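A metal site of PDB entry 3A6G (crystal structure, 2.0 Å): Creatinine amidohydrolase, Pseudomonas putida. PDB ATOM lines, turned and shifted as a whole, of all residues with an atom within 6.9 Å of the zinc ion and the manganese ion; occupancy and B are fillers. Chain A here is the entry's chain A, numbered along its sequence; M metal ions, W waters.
His 178 touches the zinc ion.
Of the 21 residues printed, 4 come within 4 Å of the zinc ion.
The nearest printed residue that does not touch the zinc ion is Glu 34 (4.2 Å).
The manganese ion is bound by OD2 of Asp 45, OE1 of Glu 34, ND1 of His 120, water W3 and water W1.
The manganese ion has five donor atoms within binding distance.
The side-chain carboxylate of Glu 183 is in hydrogen-bond range of the backbone NH of Gly 179.
ND1 of His 36 is in hydrogen-bond range of O of Glu 34 (2.7 Å).
The side-chain carboxylate of Glu 34 lies within hydrogen-bond range of the side-chain hydroxyl of Ser 74 (2.7 Å).
The side-chain carboxylate (OE1) of Glu 122 sits close to a ring nitrogen (ND1) of His 120, at 3.4 Å.
A ring nitrogen (NE2) of His 178 lies within hydrogen-bond range of the backbone carbonyl oxygen (O) of Gly 79 (3.1 Å).
NE2 of His 178 sits at hydrogen-bond distance from O of Gln 35, at 3.0 Å.
Within 4 Å of the manganese ion: Glu 34, Asp 45 and His 120.
The zinc ion is bound by the side-chain carboxylate (OD1) of Asp 45 (2.1 Å), the side-chain carboxylate (OE1) of Glu 183 (2.1 Å), water W1 (2.2 Å) and a ring nitrogen (NE2) of His 36 (2.2 Å).
The zinc ion has four donor atoms within binding distance.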
ATOM      1  N   GLY A  31      15.436  25.024 -34.036  1.00  0.00           N
ATOM      2  CA  GLY A  31      14.759  24.597 -32.832  1.00  0.00           C
ATOM      3  C   GLY A  31      14.103  25.689 -32.006  1.00  0.00           C
ATOM      4  O   GLY A  31      13.446  26.594 -32.526  1.00  0.00           O
ATOM      5  N   ALA A  32      14.289  25.583 -30.693  1.00  0.00           N
ATOM      6  CA  ALA A  32      13.706  26.535 -29.758  1.00  0.00           C
ATOM      7  C   ALA A  32      14.182  26.249 -28.338  1.00  0.00           C
ATOM      8  O   ALA A  32      14.753  25.202 -28.062  1.00  0.00           O
ATOM      9  CB  ALA A  32      12.174  26.422 -29.799  1.00  0.00           C
ATOM     10  N   GLU A  34      12.422  25.940 -25.018  1.00  0.00           N
ATOM     11  CA  GLU A  34      11.046  25.805 -24.555  1.00  0.00           C
ATOM     12  C   GLU A  34      10.902  24.774 -23.447  1.00  0.00           C
ATOM     13  O   GLU A  34      11.560  23.739 -23.457  1.00  0.00           O
ATOM     14  CB  GLU A  34      10.186  25.412 -25.762  1.00  0.00           C
ATOM     15  CG  GLU A  34       8.703  25.125 -25.493  1.00  0.00           C
ATOM     16  CD  GLU A  34       8.031  24.528 -26.718  1.00  0.00           C
ATOM     17  OE1 GLU A  34       8.610  23.583 -27.288  1.00  0.00           O
ATOM     18  OE2 GLU A  34       6.934  24.983 -27.115  1.00  0.00           O
ATOM     19  N   GLN A  35      10.024  25.067 -22.502  1.00  0.00           N
ATOM     20  CA  GLN A  35       9.780  24.171 -21.393  1.00  0.00           C
ATOM     21  C   GLN A  35       9.354  22.813 -21.942  1.00  0.00           C
ATOM     22  O   GLN A  35       8.636  22.731 -22.937  1.00  0.00           O
ATOM     23  CB  GLN A  35       8.679  24.728 -20.481  1.00  0.00           C
ATOM     24  CG  GLN A  35       7.268  24.764 -21.078  1.00  0.00           C
ATOM     25  CD  GLN A  35       6.583  23.407 -21.093  1.00  0.00           C
ATOM     26  OE1 GLN A  35       6.910  22.528 -20.301  1.00  0.00           O
ATOM     27  NE2 GLN A  35       5.600  23.242 -21.987  1.00  0.00           N
ATOM     28  N   HIS A  36       9.831  21.755 -21.298  1.00  0.00           N
ATOM     29  CA  HIS A  36       9.490  20.394 -21.691  1.00  0.00           C
ATOM     30  C   HIS A  36       9.157  19.560 -20.448  1.00  0.00           C
ATOM     31  O   HIS A  36       9.719  18.484 -20.262  1.00  0.00           O
ATOM     32  CB  HIS A  36      10.634  19.728 -22.455  1.00  0.00           C
ATOM     33  CG  HIS A  36      10.632  20.047 -23.924  1.00  0.00           C
ATOM     34  ND1 HIS A  36      11.028  21.258 -24.422  1.00  0.00           N
ATOM     35  CD2 HIS A  36      10.246  19.302 -24.987  1.00  0.00           C
ATOM     36  CE1 HIS A  36      10.892  21.258 -25.733  1.00  0.00           C
ATOM     37  NE2 HIS A  36      10.419  20.083 -26.101  1.00  0.00           N
ATOM     38  N   MET A  40      12.499  16.855 -18.299  1.00  0.00           N
ATOM     39  CA  MET A  40      13.484  17.109 -19.351  1.00  0.00           C
ATOM     40  C   MET A  40      13.937  18.574 -19.404  1.00  0.00           C
ATOM     41  O   MET A  40      13.237  19.469 -18.947  1.00  0.00           O
ATOM     42  CB  MET A  40      12.933  16.753 -20.732  1.00  0.00           C
ATOM     43  CG  MET A  40      12.772  15.297 -21.020  1.00  0.00           C
ATOM     44  SD  MET A  40      12.650  15.039 -22.800  1.00  0.00           S
ATOM     45  CE  MET A  40      11.023  15.727 -23.152  1.00  0.00           C
ATOM     46  N   VAL A  44      15.668  20.765 -25.787  1.00  0.00           N
ATOM     47  CA  VAL A  44      15.286  19.575 -26.548  1.00  0.00           C
ATOM     48  C   VAL A  44      15.031  19.822 -28.044  1.00  0.00           C
ATOM     49  O   VAL A  44      15.516  19.071 -28.886  1.00  0.00           O
ATOM     50  CB  VAL A  44      14.008  18.912 -25.945  1.00  0.00           C
ATOM     51  CG1 VAL A  44      13.460  17.839 -26.886  1.00  0.00           C
ATOM     52  CG2 VAL A  44      14.337  18.294 -24.577  1.00  0.00           C
ATOM     53  N   ASP A  45      14.281  20.867 -28.363  1.00  0.00           N
ATOM     54  CA  ASP A  45      13.966  21.177 -29.749  1.00  0.00           C
ATOM     55  C   ASP A  45      15.148  21.541 -30.629  1.00  0.00           C
ATOM     56  O   ASP A  45      15.027  21.563 -31.847  1.00  0.00           O
ATOM     57  CB  ASP A  45      12.902  22.263 -29.827  1.00  0.00           C
ATOM     58  CG  ASP A  45      11.530  21.732 -29.482  1.00  0.00           C
ATOM     59  OD1 ASP A  45      11.436  20.521 -29.195  1.00  0.00           O
ATOM     60  OD2 ASP A  45      10.561  22.515 -29.496  1.00  0.00           O
ATOM     61  N   LEU A  48      17.559  17.603 -30.519  1.00  0.00           N
ATOM     62  CA  LEU A  48      17.059  16.527 -31.364  1.00  0.00           C
ATOM     63  C   LEU A  48      17.277  16.713 -32.869  1.00  0.00           C
ATOM     64  O   LEU A  48      17.794  15.818 -33.527  1.00  0.00           O
ATOM     65  CB  LEU A  48      15.586  16.239 -31.050  1.00  0.00           C
ATOM     66  CG  LEU A  48      15.351  15.769 -29.607  1.00  0.00           C
ATOM     67  CD1 LEU A  48      13.897  15.347 -29.430  1.00  0.00           C
ATOM     68  CD2 LEU A  48      16.287  14.613 -29.273  1.00  0.00           C
ATOM     69  N   SER A  74       5.747  29.535 -28.378  1.00  0.00           N
ATOM     70  CA  SER A  74       5.109  28.267 -28.064  1.00  0.00           C
ATOM     71  C   SER A  74       3.603  28.446 -28.074  1.00  0.00           C
ATOM     72  O   SER A  74       3.076  29.424 -27.529  1.00  0.00           O
ATOM     73  CB  SER A  74       5.566  27.791 -26.673  1.00  0.00           C
ATOM     74  OG  SER A  74       4.925  26.569 -26.305  1.00  0.00           O
ATOM     75  N   SER A  78       0.357  22.824 -28.894  1.00  0.00           N
ATOM     76  CA  SER A  78       1.510  22.095 -29.392  1.00  0.00           C
ATOM     77  C   SER A  78       2.740  22.172 -28.515  1.00  0.00           C
ATOM     78  O   SER A  78       3.597  21.292 -28.549  1.00  0.00           O
ATOM     79  CB  SER A  78       1.857  22.572 -30.810  1.00  0.00           C
ATOM     80  OG  SER A  78       2.022  23.986 -30.838  1.00  0.00           O
ATOM     81  N   GLY A  79       2.847  23.235 -27.709  1.00  0.00           N
ATOM     82  CA  GLY A  79       3.999  23.375 -26.853  1.00  0.00           C
ATOM     83  C   GLY A  79       3.685  23.770 -25.426  1.00  0.00           C
ATOM     84  O   GLY A  79       4.600  23.976 -24.630  1.00  0.00           O
ATOM     85  N   GLY A 119      12.605  21.300 -35.541  1.00  0.00           N
ATOM     86  CA  GLY A 119      12.377  20.487 -34.361  1.00  0.00           C
ATOM     87  C   GLY A 119      11.307  21.070 -33.447  1.00  0.00           C
ATOM     88  O   GLY A 119      10.966  20.464 -32.431  1.00  0.00           O
ATOM     89  N   HIS A 120      10.768  22.226 -33.822  1.00  0.00           N
ATOM     90  CA  HIS A 120       9.741  22.924 -33.047  1.00  0.00           C
ATOM     91  C   HIS A 120       8.573  23.227 -33.986  1.00  0.00           C
ATOM     92  O   HIS A 120       8.667  24.096 -34.853  1.00  0.00           O
ATOM     93  CB  HIS A 120      10.352  24.233 -32.495  1.00  0.00           C
ATOM     94  CG  HIS A 120       9.413  25.072 -31.686  1.00  0.00           C
ATOM     95  ND1 HIS A 120       8.774  24.620 -30.552  1.00  0.00           N
ATOM     96  CD2 HIS A 120       9.064  26.387 -31.816  1.00  0.00           C
ATOM     97  CE1 HIS A 120       8.080  25.609 -30.008  1.00  0.00           C
ATOM     98  NE2 HIS A 120       8.238  26.688 -30.755  1.00  0.00           N
ATOM     99  N   TYR A 121       7.472  22.498 -33.809  1.00  0.00           N
ATOM    100  CA  TYR A 121       6.283  22.618 -34.653  1.00  0.00           C
ATOM    101  C   TYR A 121       5.887  24.041 -35.058  1.00  0.00           C
ATOM    102  O   TYR A 121       5.640  24.316 -36.232  1.00  0.00           O
ATOM    103  CB  TYR A 121       5.088  21.929 -33.982  1.00  0.00           C
ATOM    104  CG  TYR A 121       3.840  21.902 -34.832  1.00  0.00           C
ATOM    105  CD1 TYR A 121       3.802  21.176 -36.024  1.00  0.00           C
ATOM    106  CD2 TYR A 121       2.705  22.620 -34.464  1.00  0.00           C
ATOM    107  CE1 TYR A 121       2.660  21.159 -36.830  1.00  0.00           C
ATOM    108  CE2 TYR A 121       1.561  22.606 -35.260  1.00  0.00           C
ATOM    109  CZ  TYR A 121       1.540  21.873 -36.436  1.00  0.00           C
ATOM    110  OH  TYR A 121       0.407  21.859 -37.219  1.00  0.00           O
ATOM    111  N   GLU A 122       5.826  24.931 -34.069  1.00  0.00           N
ATOM    112  CA  GLU A 122       5.435  26.320 -34.299  1.00  0.00           C
ATOM    113  C   GLU A 122       6.306  27.120 -35.279  1.00  0.00           C
ATOM    114  O   GLU A 122       5.866  28.155 -35.784  1.00  0.00           O
ATOM    115  CB  GLU A 122       5.376  27.056 -32.953  1.00  0.00           C
ATOM    116  CG  GLU A 122       4.272  26.549 -32.014  1.00  0.00           C
ATOM    117  CD  GLU A 122       4.715  25.402 -31.119  1.00  0.00           C
ATOM    118  OE1 GLU A 122       5.523  24.549 -31.559  1.00  0.00           O
ATOM    119  OE2 GLU A 122       4.237  25.332 -29.972  1.00  0.00           O
ATOM    120  N   TYR A 153      11.735  16.410 -38.540  1.00  0.00           N
ATOM    121  CA  TYR A 153      12.199  15.045 -38.330  1.00  0.00           C
ATOM    122  C   TYR A 153      11.113  14.116 -37.804  1.00  0.00           C
ATOM    123  O   TYR A 153      11.125  12.921 -38.103  1.00  0.00           O
ATOM    124  CB  TYR A 153      13.414  15.057 -37.380  1.00  0.00           C
ATOM    125  CG  TYR A 153      13.064  15.245 -35.920  1.00  0.00           C
ATOM    126  CD1 TYR A 153      12.510  14.200 -35.190  1.00  0.00           C
ATOM    127  CD2 TYR A 153      13.261  16.477 -35.284  1.00  0.00           C
ATOM    128  CE1 TYR A 153      12.163  14.365 -33.860  1.00  0.00           C
ATOM    129  CE2 TYR A 153      12.905  16.652 -33.948  1.00  0.00           C
ATOM    130  CZ  TYR A 153      12.357  15.587 -33.244  1.00  0.00           C
ATOM    131  OH  TYR A 153      11.995  15.723 -31.923  1.00  0.00           O
ATOM    132  N   GLU A 177       2.227  15.159 -28.712  1.00  0.00           N
ATOM    133  CA  GLU A 177       3.564  14.707 -28.393  1.00  0.00           C
ATOM    134  C   GLU A 177       4.567  15.762 -27.926  1.00  0.00           C
ATOM    135  O   GLU A 177       5.726  15.747 -28.348  1.00  0.00           O
ATOM    136  CB  GLU A 177       4.155  13.952 -29.597  1.00  0.00           C
ATOM    137  CG  GLU A 177       3.765  12.486 -29.676  1.00  0.00           C
ATOM    138  CD  GLU A 177       4.206  11.701 -28.446  1.00  0.00           C
ATOM    139  OE1 GLU A 177       5.353  11.894 -27.989  1.00  0.00           O
ATOM    140  OE2 GLU A 177       3.417  10.873 -27.943  1.00  0.00           O
ATOM    141  N   HIS A 178       4.136  16.696 -27.077  1.00  0.00           N
ATOM    142  CA  HIS A 178       5.076  17.683 -26.549  1.00  0.00           C
ATOM    143  C   HIS A 178       5.507  17.177 -25.179  1.00  0.00           C
ATOM    144  O   HIS A 178       4.691  17.104 -24.259  1.00  0.00           O
ATOM    145  CB  HIS A 178       4.433  19.059 -26.396  1.00  0.00           C
ATOM    146  CG  HIS A 178       5.323  20.044 -25.701  1.00  0.00           C
ATOM    147  ND1 HIS A 178       6.513  20.496 -26.242  1.00  0.00           N
ATOM    148  CD2 HIS A 178       5.228  20.632 -24.481  1.00  0.00           C
ATOM    149  CE1 HIS A 178       7.108  21.305 -25.382  1.00  0.00           C
ATOM    150  NE2 HIS A 178       6.345  21.406 -24.307  1.00  0.00           N
ATOM    151  N   GLY A 179       6.773  16.806 -25.052  1.00  0.00           N
ATOM    152  CA  GLY A 179       7.297  16.308 -23.787  1.00  0.00           C
ATOM    153  C   GLY A 179       6.768  14.924 -23.444  1.00  0.00           C
ATOM    154  O   GLY A 179       6.851  14.489 -22.298  1.00  0.00           O
ATOM    155  N   GLU A 183       9.585  12.439 -27.819  1.00  0.00           N
ATOM    156  CA  GLU A 183      10.767  13.235 -27.519  1.00  0.00           C
ATOM    157  C   GLU A 183      11.578  12.701 -26.356  1.00  0.00           C
ATOM    158  O   GLU A 183      12.805  12.698 -26.385  1.00  0.00           O
ATOM    159  CB  GLU A 183      10.369  14.683 -27.217  1.00  0.00           C
ATOM    160  CG  GLU A 183       9.646  15.374 -28.338  1.00  0.00           C
ATOM    161  CD  GLU A 183       9.434  16.836 -28.046  1.00  0.00           C
ATOM    162  OE1 GLU A 183      10.059  17.655 -28.744  1.00  0.00           O
ATOM    163  OE2 GLU A 183       8.665  17.156 -27.122  1.00  0.00           O
HETATM  164 ZN    ZN M   1       9.855  19.654 -28.141  1.00  0.00          ZN
HETATM  165 MN    MN M   2       8.540  22.771 -29.268  1.00  0.00          MN
HETATM  166  O   HOH W   1       7.996  20.638 -28.598  1.00  0.00           O
HETATM  167  O   HOH W   2       7.817  20.427 -31.093  1.00  0.00           O
HETATM  168  O   HOH W   3       6.279  23.074 -29.212  1.00  0.00           O
